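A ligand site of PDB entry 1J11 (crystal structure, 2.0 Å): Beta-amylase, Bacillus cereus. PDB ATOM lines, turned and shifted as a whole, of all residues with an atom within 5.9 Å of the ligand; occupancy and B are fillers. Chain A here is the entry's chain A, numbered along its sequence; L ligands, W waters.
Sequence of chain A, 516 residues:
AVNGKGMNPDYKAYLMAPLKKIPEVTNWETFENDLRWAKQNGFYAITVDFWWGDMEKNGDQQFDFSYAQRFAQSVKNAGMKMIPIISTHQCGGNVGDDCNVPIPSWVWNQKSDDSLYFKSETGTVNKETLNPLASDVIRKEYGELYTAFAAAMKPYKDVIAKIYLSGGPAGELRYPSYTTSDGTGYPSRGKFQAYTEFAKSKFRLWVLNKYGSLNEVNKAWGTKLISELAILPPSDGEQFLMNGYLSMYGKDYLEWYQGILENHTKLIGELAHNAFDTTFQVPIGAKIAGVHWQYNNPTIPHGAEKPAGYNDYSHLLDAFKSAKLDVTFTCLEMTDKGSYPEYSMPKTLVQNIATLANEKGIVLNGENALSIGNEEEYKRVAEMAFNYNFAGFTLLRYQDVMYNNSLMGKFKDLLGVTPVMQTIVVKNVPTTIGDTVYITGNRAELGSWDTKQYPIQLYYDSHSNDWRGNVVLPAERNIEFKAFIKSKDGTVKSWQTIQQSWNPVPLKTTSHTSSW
Water W5 lies within hydrogen-bond range of an oxygen (O6) of the ligand (2.7 Å), the side-chain hydroxyl of Thr 47 (3.2 Å), the guanidinium group of Arg 397 (3.4 Å) and the side-chain sulfur of Met 16 (3.7 Å).
Water W2 lies within hydrogen-bond range of an oxygen (O4) of the ligand, the side-chain amino group of Lys 287 and the backbone carbonyl oxygen of Ala 170.
Water W1 bridges the backbone carbonyl oxygen of Val 95 (2.9 Å) and an oxygen (O2) of the ligand (3.1 Å).
Water W3 lies within hydrogen-bond range of OD2 of Asp 97, O of Val 95 and O2 of the ligand.
The side-chain amino group (NZ) of Lys 287 lies within salt-bridge range of the side-chain carboxylate (OE2) of Glu 367.
The guanidinium group of Arg 397 sits at hydrogen-bond distance from the backbone carbonyl oxygen of Ala 17, at 3.0 Å.
ND1 of His 89 is in hydrogen-bond range of N of Gly 171.
OD1 of Asp 49 lies within hydrogen-bond range of OG of Ser 87 (2.8 Å).
NE1 of Trp 51 is in hydrogen-bond range of O of Leu 19 (3.2 Å).
SD of Met 16 lies close to NH1 of Arg 397, 3.7 Å away.
The side-chain carboxylate of Asp 97 is in hydrogen-bond range of the backbone NH of Asn 94 (3.3 Å).
N of Gly 92 is in hydrogen-bond range of OD1 of Asp 97.
OE1 of Glu 367 sits close to O7 of the ligand (3.1 Å).
Leu 19 touches the ligand (CD1 to O6, 3.8 Å).
Trp 51 touches the ligand.
Asn 94 touches the ligand (CB to O2, 3.7 Å).
Ala 170 touches the ligand.
Hydrophobic or aromatic side chains that line the ligand: Met 16, Leu 19, Trp 51, His 89 and Ala 170.
The nearest printed residue that does not touch the ligand is Leu 396 (4.1 Å).
An oxygen (O2) of the ligand sits at hydrogen-bond distance from the side-chain carboxylate (OD2) of Asp 97 (2.5 Å).
O6 of the ligand lies within hydrogen-bond range of SD of Met 16.
NE2 of His 89 sits at hydrogen-bond distance from O3 of the ligand (2.8 Å).
C9 of the ligand is bonded to OE2 of Glu 172 (1.4 Å).
An oxygen (O5) of the ligand lies within hydrogen-bond range of the guanidinium group (NH2) of Arg 397.
The side-chain carboxylate of Asp 49 lies within hydrogen-bond range of an oxygen (O6) of the ligand (2.7 Å).
The side-chain amino group of Lys 287 lies within hydrogen-bond range of an oxygen (O7) of the ligand (3.2 Å).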
ATOM      1  N   MET A  16      -7.841 -10.228   2.234  1.00  0.00           N
ATOM      2  CA  MET A  16      -7.226  -9.683   3.434  1.00  0.00           C
ATOM      3  C   MET A  16      -6.021  -8.840   3.096  1.00  0.00           C
ATOM      4  O   MET A  16      -5.158  -9.257   2.319  1.00  0.00           O
ATOM      5  CB  MET A  16      -6.805 -10.804   4.378  1.00  0.00           C
ATOM      6  CG  MET A  16      -7.941 -11.435   5.125  1.00  0.00           C
ATOM      7  SD  MET A  16      -7.349 -12.400   6.514  1.00  0.00           S
ATOM      8  CE  MET A  16      -8.763 -13.402   6.816  1.00  0.00           C
ATOM      9  N   ALA A  17      -5.971  -7.652   3.679  1.00  0.00           N
ATOM     10  CA  ALA A  17      -4.855  -6.742   3.462  1.00  0.00           C
ATOM     11  C   ALA A  17      -3.699  -7.221   4.326  1.00  0.00           C
ATOM     12  O   ALA A  17      -3.871  -8.107   5.177  1.00  0.00           O
ATOM     13  CB  ALA A  17      -5.263  -5.336   3.880  1.00  0.00           C
ATOM     14  N   LEU A  19      -0.816  -7.397   7.248  1.00  0.00           N
ATOM     15  CA  LEU A  19      -0.916  -7.132   8.695  1.00  0.00           C
ATOM     16  C   LEU A  19      -0.211  -5.814   9.034  1.00  0.00           C
ATOM     17  O   LEU A  19      -0.618  -5.086   9.950  1.00  0.00           O
ATOM     18  CB  LEU A  19      -0.286  -8.291   9.496  1.00  0.00           C
ATOM     19  CG  LEU A  19      -1.148  -9.382  10.148  1.00  0.00           C
ATOM     20  CD1 LEU A  19      -2.595  -9.346   9.706  1.00  0.00           C
ATOM     21  CD2 LEU A  19      -0.509 -10.735   9.886  1.00  0.00           C
ATOM     22  N   THR A  47     -10.448  -6.525   3.284  1.00  0.00           N
ATOM     23  CA  THR A  47     -10.645  -6.453   4.735  1.00  0.00           C
ATOM     24  C   THR A  47      -9.317  -5.958   5.301  1.00  0.00           C
ATOM     25  O   THR A  47      -8.240  -6.330   4.817  1.00  0.00           O
ATOM     26  CB  THR A  47     -11.068  -7.824   5.370  1.00  0.00           C
ATOM     27  OG1 THR A  47      -9.965  -8.752   5.335  1.00  0.00           O
ATOM     28  CG2 THR A  47     -12.241  -8.442   4.633  1.00  0.00           C
ATOM     29  N   ASP A  49      -7.102  -4.677   9.019  1.00  0.00           N
ATOM     30  CA  ASP A  49      -6.974  -4.519  10.462  1.00  0.00           C
ATOM     31  C   ASP A  49      -6.517  -3.121  10.822  1.00  0.00           C
ATOM     32  O   ASP A  49      -5.483  -2.650  10.343  1.00  0.00           O
ATOM     33  CB  ASP A  49      -5.926  -5.476  11.045  1.00  0.00           C
ATOM     34  CG  ASP A  49      -6.334  -6.922  10.978  1.00  0.00           C
ATOM     35  OD1 ASP A  49      -7.243  -7.335  11.741  1.00  0.00           O
ATOM     36  OD2 ASP A  49      -5.721  -7.655  10.172  1.00  0.00           O
ATOM     37  N   TRP A  51      -5.382  -1.487  13.954  1.00  0.00           N
ATOM     38  CA  TRP A  51      -4.957  -1.833  15.297  1.00  0.00           C
ATOM     39  C   TRP A  51      -5.209  -0.832  16.408  1.00  0.00           C
ATOM     40  O   TRP A  51      -4.867   0.355  16.281  1.00  0.00           O
ATOM     41  CB  TRP A  51      -3.467  -2.220  15.278  1.00  0.00           C
ATOM     42  CG  TRP A  51      -3.177  -3.284  14.286  1.00  0.00           C
ATOM     43  CD1 TRP A  51      -2.532  -3.144  13.090  1.00  0.00           C
ATOM     44  CD2 TRP A  51      -3.565  -4.659  14.366  1.00  0.00           C
ATOM     45  NE1 TRP A  51      -2.497  -4.346  12.422  1.00  0.00           N
ATOM     46  CE2 TRP A  51      -3.122  -5.295  13.180  1.00  0.00           C
ATOM     47  CE3 TRP A  51      -4.240  -5.428  15.325  1.00  0.00           C
ATOM     48  CZ2 TRP A  51      -3.347  -6.653  12.937  1.00  0.00           C
ATOM     49  CZ3 TRP A  51      -4.465  -6.766  15.076  1.00  0.00           C
ATOM     50  CH2 TRP A  51      -4.025  -7.371  13.890  1.00  0.00           C
ATOM     51  N   ILE A  85     -11.592  -3.802  10.215  1.00  0.00           N
ATOM     52  CA  ILE A  85     -11.689  -4.665  11.378  1.00  0.00           C
ATOM     53  C   ILE A  85     -11.150  -3.808  12.513  1.00  0.00           C
ATOM     54  O   ILE A  85      -9.993  -3.365  12.472  1.00  0.00           O
ATOM     55  CB  ILE A  85     -10.820  -5.938  11.231  1.00  0.00           C
ATOM     56  CG1 ILE A  85     -11.217  -6.706   9.960  1.00  0.00           C
ATOM     57  CG2 ILE A  85     -10.948  -6.818  12.472  1.00  0.00           C
ATOM     58  CD1 ILE A  85     -10.220  -7.771   9.563  1.00  0.00           C
ATOM     59  N   SER A  87      -9.565  -3.828  15.300  1.00  0.00           N
ATOM     60  CA  SER A  87      -8.724  -4.764  16.010  1.00  0.00           C
ATOM     61  C   SER A  87      -8.276  -4.414  17.411  1.00  0.00           C
ATOM     62  O   SER A  87      -7.140  -3.962  17.620  1.00  0.00           O
ATOM     63  CB  SER A  87      -7.539  -5.145  15.136  1.00  0.00           C
ATOM     64  OG  SER A  87      -7.991  -5.727  13.927  1.00  0.00           O
ATOM     65  N   HIS A  89      -7.299  -6.341  19.437  1.00  0.00           N
ATOM     66  CA  HIS A  89      -6.442  -7.463  19.808  1.00  0.00           C
ATOM     67  C   HIS A  89      -5.015  -7.189  19.346  1.00  0.00           C
ATOM     68  O   HIS A  89      -4.775  -6.301  18.521  1.00  0.00           O
ATOM     69  CB  HIS A  89      -6.995  -8.800  19.232  1.00  0.00           C
ATOM     70  CG  HIS A  89      -6.954  -8.897  17.727  1.00  0.00           C
ATOM     71  ND1 HIS A  89      -7.998  -8.487  16.924  1.00  0.00           N
ATOM     72  CD2 HIS A  89      -6.004  -9.381  16.892  1.00  0.00           C
ATOM     73  CE1 HIS A  89      -7.687  -8.716  15.648  1.00  0.00           C
ATOM     74  NE2 HIS A  89      -6.488  -9.262  15.609  1.00  0.00           N
ATOM     75  N   GLN A  90      -4.059  -7.934  19.884  1.00  0.00           N
ATOM     76  CA  GLN A  90      -2.660  -7.763  19.528  1.00  0.00           C
ATOM     77  C   GLN A  90      -2.241  -8.429  18.223  1.00  0.00           C
ATOM     78  O   GLN A  90      -2.619  -9.568  17.962  1.00  0.00           O
ATOM     79  CB  GLN A  90      -1.783  -8.298  20.646  1.00  0.00           C
ATOM     80  CG  GLN A  90      -0.319  -8.357  20.285  1.00  0.00           C
ATOM     81  CD  GLN A  90       0.476  -9.097  21.307  1.00  0.00           C
ATOM     82  OE1 GLN A  90       0.521  -8.699  22.466  1.00  0.00           O
ATOM     83  NE2 GLN A  90       1.095 -10.211  20.912  1.00  0.00           N
ATOM     84  N   CYS A  91      -1.447  -7.738  17.425  1.00  0.00           N
ATOM     85  CA  CYS A  91      -0.936  -8.316  16.182  1.00  0.00           C
ATOM     86  C   CYS A  91       0.437  -8.866  16.546  1.00  0.00           C
ATOM     87  O   CYS A  91       1.271  -8.168  17.129  1.00  0.00           O
ATOM     88  CB  CYS A  91      -0.793  -7.273  15.077  1.00  0.00           C
ATOM     89  SG  CYS A  91      -0.584  -8.006  13.413  1.00  0.00           S
ATOM     90  N   GLY A  92       0.672 -10.115  16.181  1.00  0.00           N
ATOM     91  CA  GLY A  92       1.933 -10.762  16.496  1.00  0.00           C
ATOM     92  C   GLY A  92       1.619 -11.873  17.485  1.00  0.00           C
ATOM     93  O   GLY A  92       0.815 -11.680  18.404  1.00  0.00           O
ATOM     94  N   ASN A  94       0.151 -14.943  16.714  1.00  0.00           N
ATOM     95  CA  ASN A  94      -0.754 -15.941  16.161  1.00  0.00           C
ATOM     96  C   ASN A  94      -0.220 -16.511  14.843  1.00  0.00           C
ATOM     97  O   ASN A  94       0.724 -15.963  14.259  1.00  0.00           O
ATOM     98  CB  ASN A  94      -2.157 -15.383  16.014  1.00  0.00           C
ATOM     99  CG  ASN A  94      -2.859 -15.203  17.355  1.00  0.00           C
ATOM    100  OD1 ASN A  94      -3.010 -14.082  17.831  1.00  0.00           O
ATOM    101  ND2 ASN A  94      -3.277 -16.301  17.953  1.00  0.00           N
ATOM    102  N   VAL A  95      -0.792 -17.618  14.390  1.00  0.00           N
ATOM    103  CA  VAL A  95      -0.338 -18.256  13.164  1.00  0.00           C
ATOM    104  C   VAL A  95      -0.431 -17.355  11.922  1.00  0.00           C
ATOM    105  O   VAL A  95      -1.513 -16.932  11.513  1.00  0.00           O
ATOM    106  CB  VAL A  95      -1.023 -19.627  12.917  1.00  0.00           C
ATOM    107  CG1 VAL A  95      -2.518 -19.452  12.679  1.00  0.00           C
ATOM    108  CG2 VAL A  95      -0.365 -20.345  11.740  1.00  0.00           C
ATOM    109  N   GLY A  96       0.739 -17.065  11.354  1.00  0.00           N
ATOM    110  CA  GLY A  96       0.807 -16.220  10.173  1.00  0.00           C
ATOM    111  C   GLY A  96       1.042 -14.754  10.486  1.00  0.00           C
ATOM    112  O   GLY A  96       1.160 -13.934   9.570  1.00  0.00           O
ATOM    113  N   ASP A  97       1.126 -14.420  11.763  1.00  0.00           N
ATOM    114  CA  ASP A  97       1.342 -13.041  12.167  1.00  0.00           C
ATOM    115  C   ASP A  97       2.753 -12.518  11.948  1.00  0.00           C
ATOM    116  O   ASP A  97       3.704 -12.940  12.602  1.00  0.00           O
ATOM    117  CB  ASP A  97       0.955 -12.836  13.635  1.00  0.00           C
ATOM    118  CG  ASP A  97      -0.545 -12.728  13.830  1.00  0.00           C
ATOM    119  OD1 ASP A  97      -0.975 -12.417  14.956  1.00  0.00           O
ATOM    120  OD2 ASP A  97      -1.291 -12.949  12.864  1.00  0.00           O
ATOM    121  N   PRO A 169      -8.820 -12.953  20.872  1.00  0.00           N
ATOM    122  CA  PRO A 169      -7.494 -13.221  20.286  1.00  0.00           C
ATOM    123  C   PRO A 169      -7.584 -13.462  18.778  1.00  0.00           C
ATOM    124  O   PRO A 169      -8.492 -14.159  18.306  1.00  0.00           O
ATOM    125  CB  PRO A 169      -7.035 -14.485  21.017  1.00  0.00           C
ATOM    126  CG  PRO A 169      -7.796 -14.439  22.313  1.00  0.00           C
ATOM    127  CD  PRO A 169      -9.158 -14.002  21.861  1.00  0.00           C
ATOM    128  N   ALA A 170      -6.645 -12.883  18.036  1.00  0.00           N
ATOM    129  CA  ALA A 170      -6.593 -13.018  16.575  1.00  0.00           C
ATOM    130  C   ALA A 170      -7.889 -12.538  15.923  1.00  0.00           C
ATOM    131  O   ALA A 170      -8.141 -12.832  14.759  1.00  0.00           O
ATOM    132  CB  ALA A 170      -6.285 -14.455  16.172  1.00  0.00           C
ATOM    133  N   GLY A 171      -8.701 -11.791  16.669  1.00  0.00           N
ATOM    134  CA  GLY A 171      -9.953 -11.281  16.136  1.00  0.00           C
ATOM    135  C   GLY A 171     -11.163 -12.197  16.222  1.00  0.00           C
ATOM    136  O   GLY A 171     -12.225 -11.851  15.703  1.00  0.00           O
ATOM    137  N   GLU A 172     -11.020 -13.339  16.892  1.00  0.00           N
ATOM    138  CA  GLU A 172     -12.140 -14.268  17.021  1.00  0.00           C
ATOM    139  C   GLU A 172     -12.710 -14.305  18.420  1.00  0.00           C
ATOM    140  O   GLU A 172     -11.992 -14.115  19.395  1.00  0.00           O
ATOM    141  CB  GLU A 172     -11.693 -15.678  16.617  1.00  0.00           C
ATOM    142  CG  GLU A 172     -11.341 -15.797  15.160  1.00  0.00           C
ATOM    143  CD  GLU A 172      -9.880 -16.066  14.931  1.00  0.00           C
ATOM    144  OE1 GLU A 172      -9.189 -16.520  15.842  1.00  0.00           O
ATOM    145  OE2 GLU A 172      -9.363 -15.763  13.673  1.00  0.00           O
ATOM    146  N   LYS A 287     -16.185 -13.000  14.319  1.00  0.00           N
ATOM    147  CA  LYS A 287     -15.704 -14.332  13.955  1.00  0.00           C
ATOM    148  C   LYS A 287     -15.683 -15.406  15.037  1.00  0.00           C
ATOM    149  O   LYS A 287     -15.522 -15.118  16.229  1.00  0.00           O
ATOM    150  CB  LYS A 287     -14.302 -14.208  13.360  1.00  0.00           C
ATOM    151  CG  LYS A 287     -14.158 -13.092  12.348  1.00  0.00           C
ATOM    152  CD  LYS A 287     -12.738 -12.992  11.837  1.00  0.00           C
ATOM    153  CE  LYS A 287     -12.620 -11.910  10.792  1.00  0.00           C
ATOM    154  NZ  LYS A 287     -11.278 -11.932  10.179  1.00  0.00           N
ATOM    155  N   THR A 330     -13.903 -19.810   9.999  1.00  0.00           N
ATOM    156  CA  THR A 330     -12.662 -20.060   9.285  1.00  0.00           C
ATOM    157  C   THR A 330     -12.522 -21.537   8.884  1.00  0.00           C
ATOM    158  O   THR A 330     -13.425 -22.339   9.143  1.00  0.00           O
ATOM    159  CB  THR A 330     -11.475 -19.616  10.164  1.00  0.00           C
ATOM    160  OG1 THR A 330     -11.378 -20.491  11.292  1.00  0.00           O
ATOM    161  CG2 THR A 330     -11.697 -18.204  10.698  1.00  0.00           C
ATOM    162  N   GLU A 367     -13.690 -18.028   5.745  1.00  0.00           N
ATOM    163  CA  GLU A 367     -12.332 -17.672   5.377  1.00  0.00           C
ATOM    164  C   GLU A 367     -11.403 -18.862   5.565  1.00  0.00           C
ATOM    165  O   GLU A 367     -11.725 -19.821   6.282  1.00  0.00           O
ATOM    166  CB  GLU A 367     -11.843 -16.422   6.147  1.00  0.00           C
ATOM    167  CG  GLU A 367     -11.780 -16.543   7.646  1.00  0.00           C
ATOM    168  CD  GLU A 367     -11.380 -15.245   8.320  1.00  0.00           C
ATOM    169  OE1 GLU A 367     -10.368 -15.242   9.038  1.00  0.00           O
ATOM    170  OE2 GLU A 367     -12.078 -14.230   8.142  1.00  0.00           O
ATOM    171  N   ALA A 369      -8.060 -20.851   6.772  1.00  0.00           N
ATOM    172  CA  ALA A 369      -7.234 -20.784   7.963  1.00  0.00           C
ATOM    173  C   ALA A 369      -5.784 -20.486   7.631  1.00  0.00           C
ATOM    174  O   ALA A 369      -5.173 -19.612   8.237  1.00  0.00           O
ATOM    175  CB  ALA A 369      -7.347 -22.079   8.751  1.00  0.00           C
ATOM    176  N   LEU A 396      -7.131 -15.183   2.772  1.00  0.00           N
ATOM    177  CA  LEU A 396      -5.964 -14.809   3.536  1.00  0.00           C
ATOM    178  C   LEU A 396      -4.827 -15.390   2.671  1.00  0.00           C
ATOM    179  O   LEU A 396      -4.800 -16.604   2.440  1.00  0.00           O
ATOM    180  CB  LEU A 396      -6.011 -15.492   4.918  1.00  0.00           C
ATOM    181  CG  LEU A 396      -4.838 -15.365   5.890  1.00  0.00           C
ATOM    182  CD1 LEU A 396      -5.290 -15.693   7.319  1.00  0.00           C
ATOM    183  CD2 LEU A 396      -3.680 -16.261   5.468  1.00  0.00           C
ATOM    184  N   ARG A 397      -3.905 -14.561   2.173  1.00  0.00           N
ATOM    185  CA  ARG A 397      -3.875 -13.124   2.398  1.00  0.00           C
ATOM    186  C   ARG A 397      -3.252 -12.447   1.171  1.00  0.00           C
ATOM    187  O   ARG A 397      -2.547 -13.082   0.392  1.00  0.00           O
ATOM    188  CB  ARG A 397      -3.026 -12.799   3.632  1.00  0.00           C
ATOM    189  CG  ARG A 397      -3.006 -11.321   4.012  1.00  0.00           C
ATOM    190  CD  ARG A 397      -2.122 -11.064   5.229  1.00  0.00           C
ATOM    191  NE  ARG A 397      -2.555 -11.837   6.394  1.00  0.00           N
ATOM    192  CZ  ARG A 397      -3.544 -11.507   7.213  1.00  0.00           C
ATOM    193  NH1 ARG A 397      -4.248 -10.392   7.023  1.00  0.00           N
ATOM    194  NH2 ARG A 397      -3.831 -12.284   8.252  1.00  0.00           N
HETATM  195  C1  LIG L   1      -5.188 -13.279  11.393  1.00  0.00           C
HETATM  196  O1  LIG L   1      -6.267 -14.041  11.923  1.00  0.00           O
HETATM  197  C2  LIG L   1      -4.403 -12.460  12.440  1.00  0.00           C
HETATM  198  O2  LIG L   1      -3.752 -13.276  13.415  1.00  0.00           O
HETATM  199  C3  LIG L   1      -5.375 -11.499  13.095  1.00  0.00           C
HETATM  200  O3  LIG L   1      -4.715 -10.679  14.038  1.00  0.00           O
HETATM  201  C4  LIG L   1      -6.086 -10.633  12.057  1.00  0.00           C
HETATM  202  O4  LIG L   1      -7.123  -9.910  12.702  1.00  0.00           O
HETATM  203  C5  LIG L   1      -6.695 -11.504  10.955  1.00  0.00           C
HETATM  204  O5  LIG L   1      -5.703 -12.395  10.415  1.00  0.00           O
HETATM  205  C6  LIG L   1      -7.288 -10.710   9.812  1.00  0.00           C
HETATM  206  O6  LIG L   1      -6.288 -10.013   9.098  1.00  0.00           O
HETATM  207  C7  LIG L   1      -6.937 -14.850  10.986  1.00  0.00           C
HETATM  208  C8  LIG L   1      -8.338 -15.103  11.507  1.00  0.00           C
HETATM  209  C9  LIG L   1      -8.211 -15.689  12.900  1.00  0.00           C
HETATM  210  O7  LIG L   1      -9.079 -13.870  11.549  1.00  0.00           O
HETATM  211  O   HOH W   1      -3.608 -16.407  13.495  1.00  0.00           O
HETATM  212  O   HOH W   2      -9.700 -10.935  12.568  1.00  0.00           O
HETATM  213  O   HOH W   3      -2.186 -14.255  10.652  1.00  0.00           O
HETATM  214  O   HOH W   4      -8.746 -17.345   8.917  1.00  0.00           O
HETATM  215  O   HOH W   5      -7.167  -8.710   6.893  1.00  0.00           O
HETATM  216  O   HOH W   6      -3.260 -11.530  16.183  1.00  0.00           O
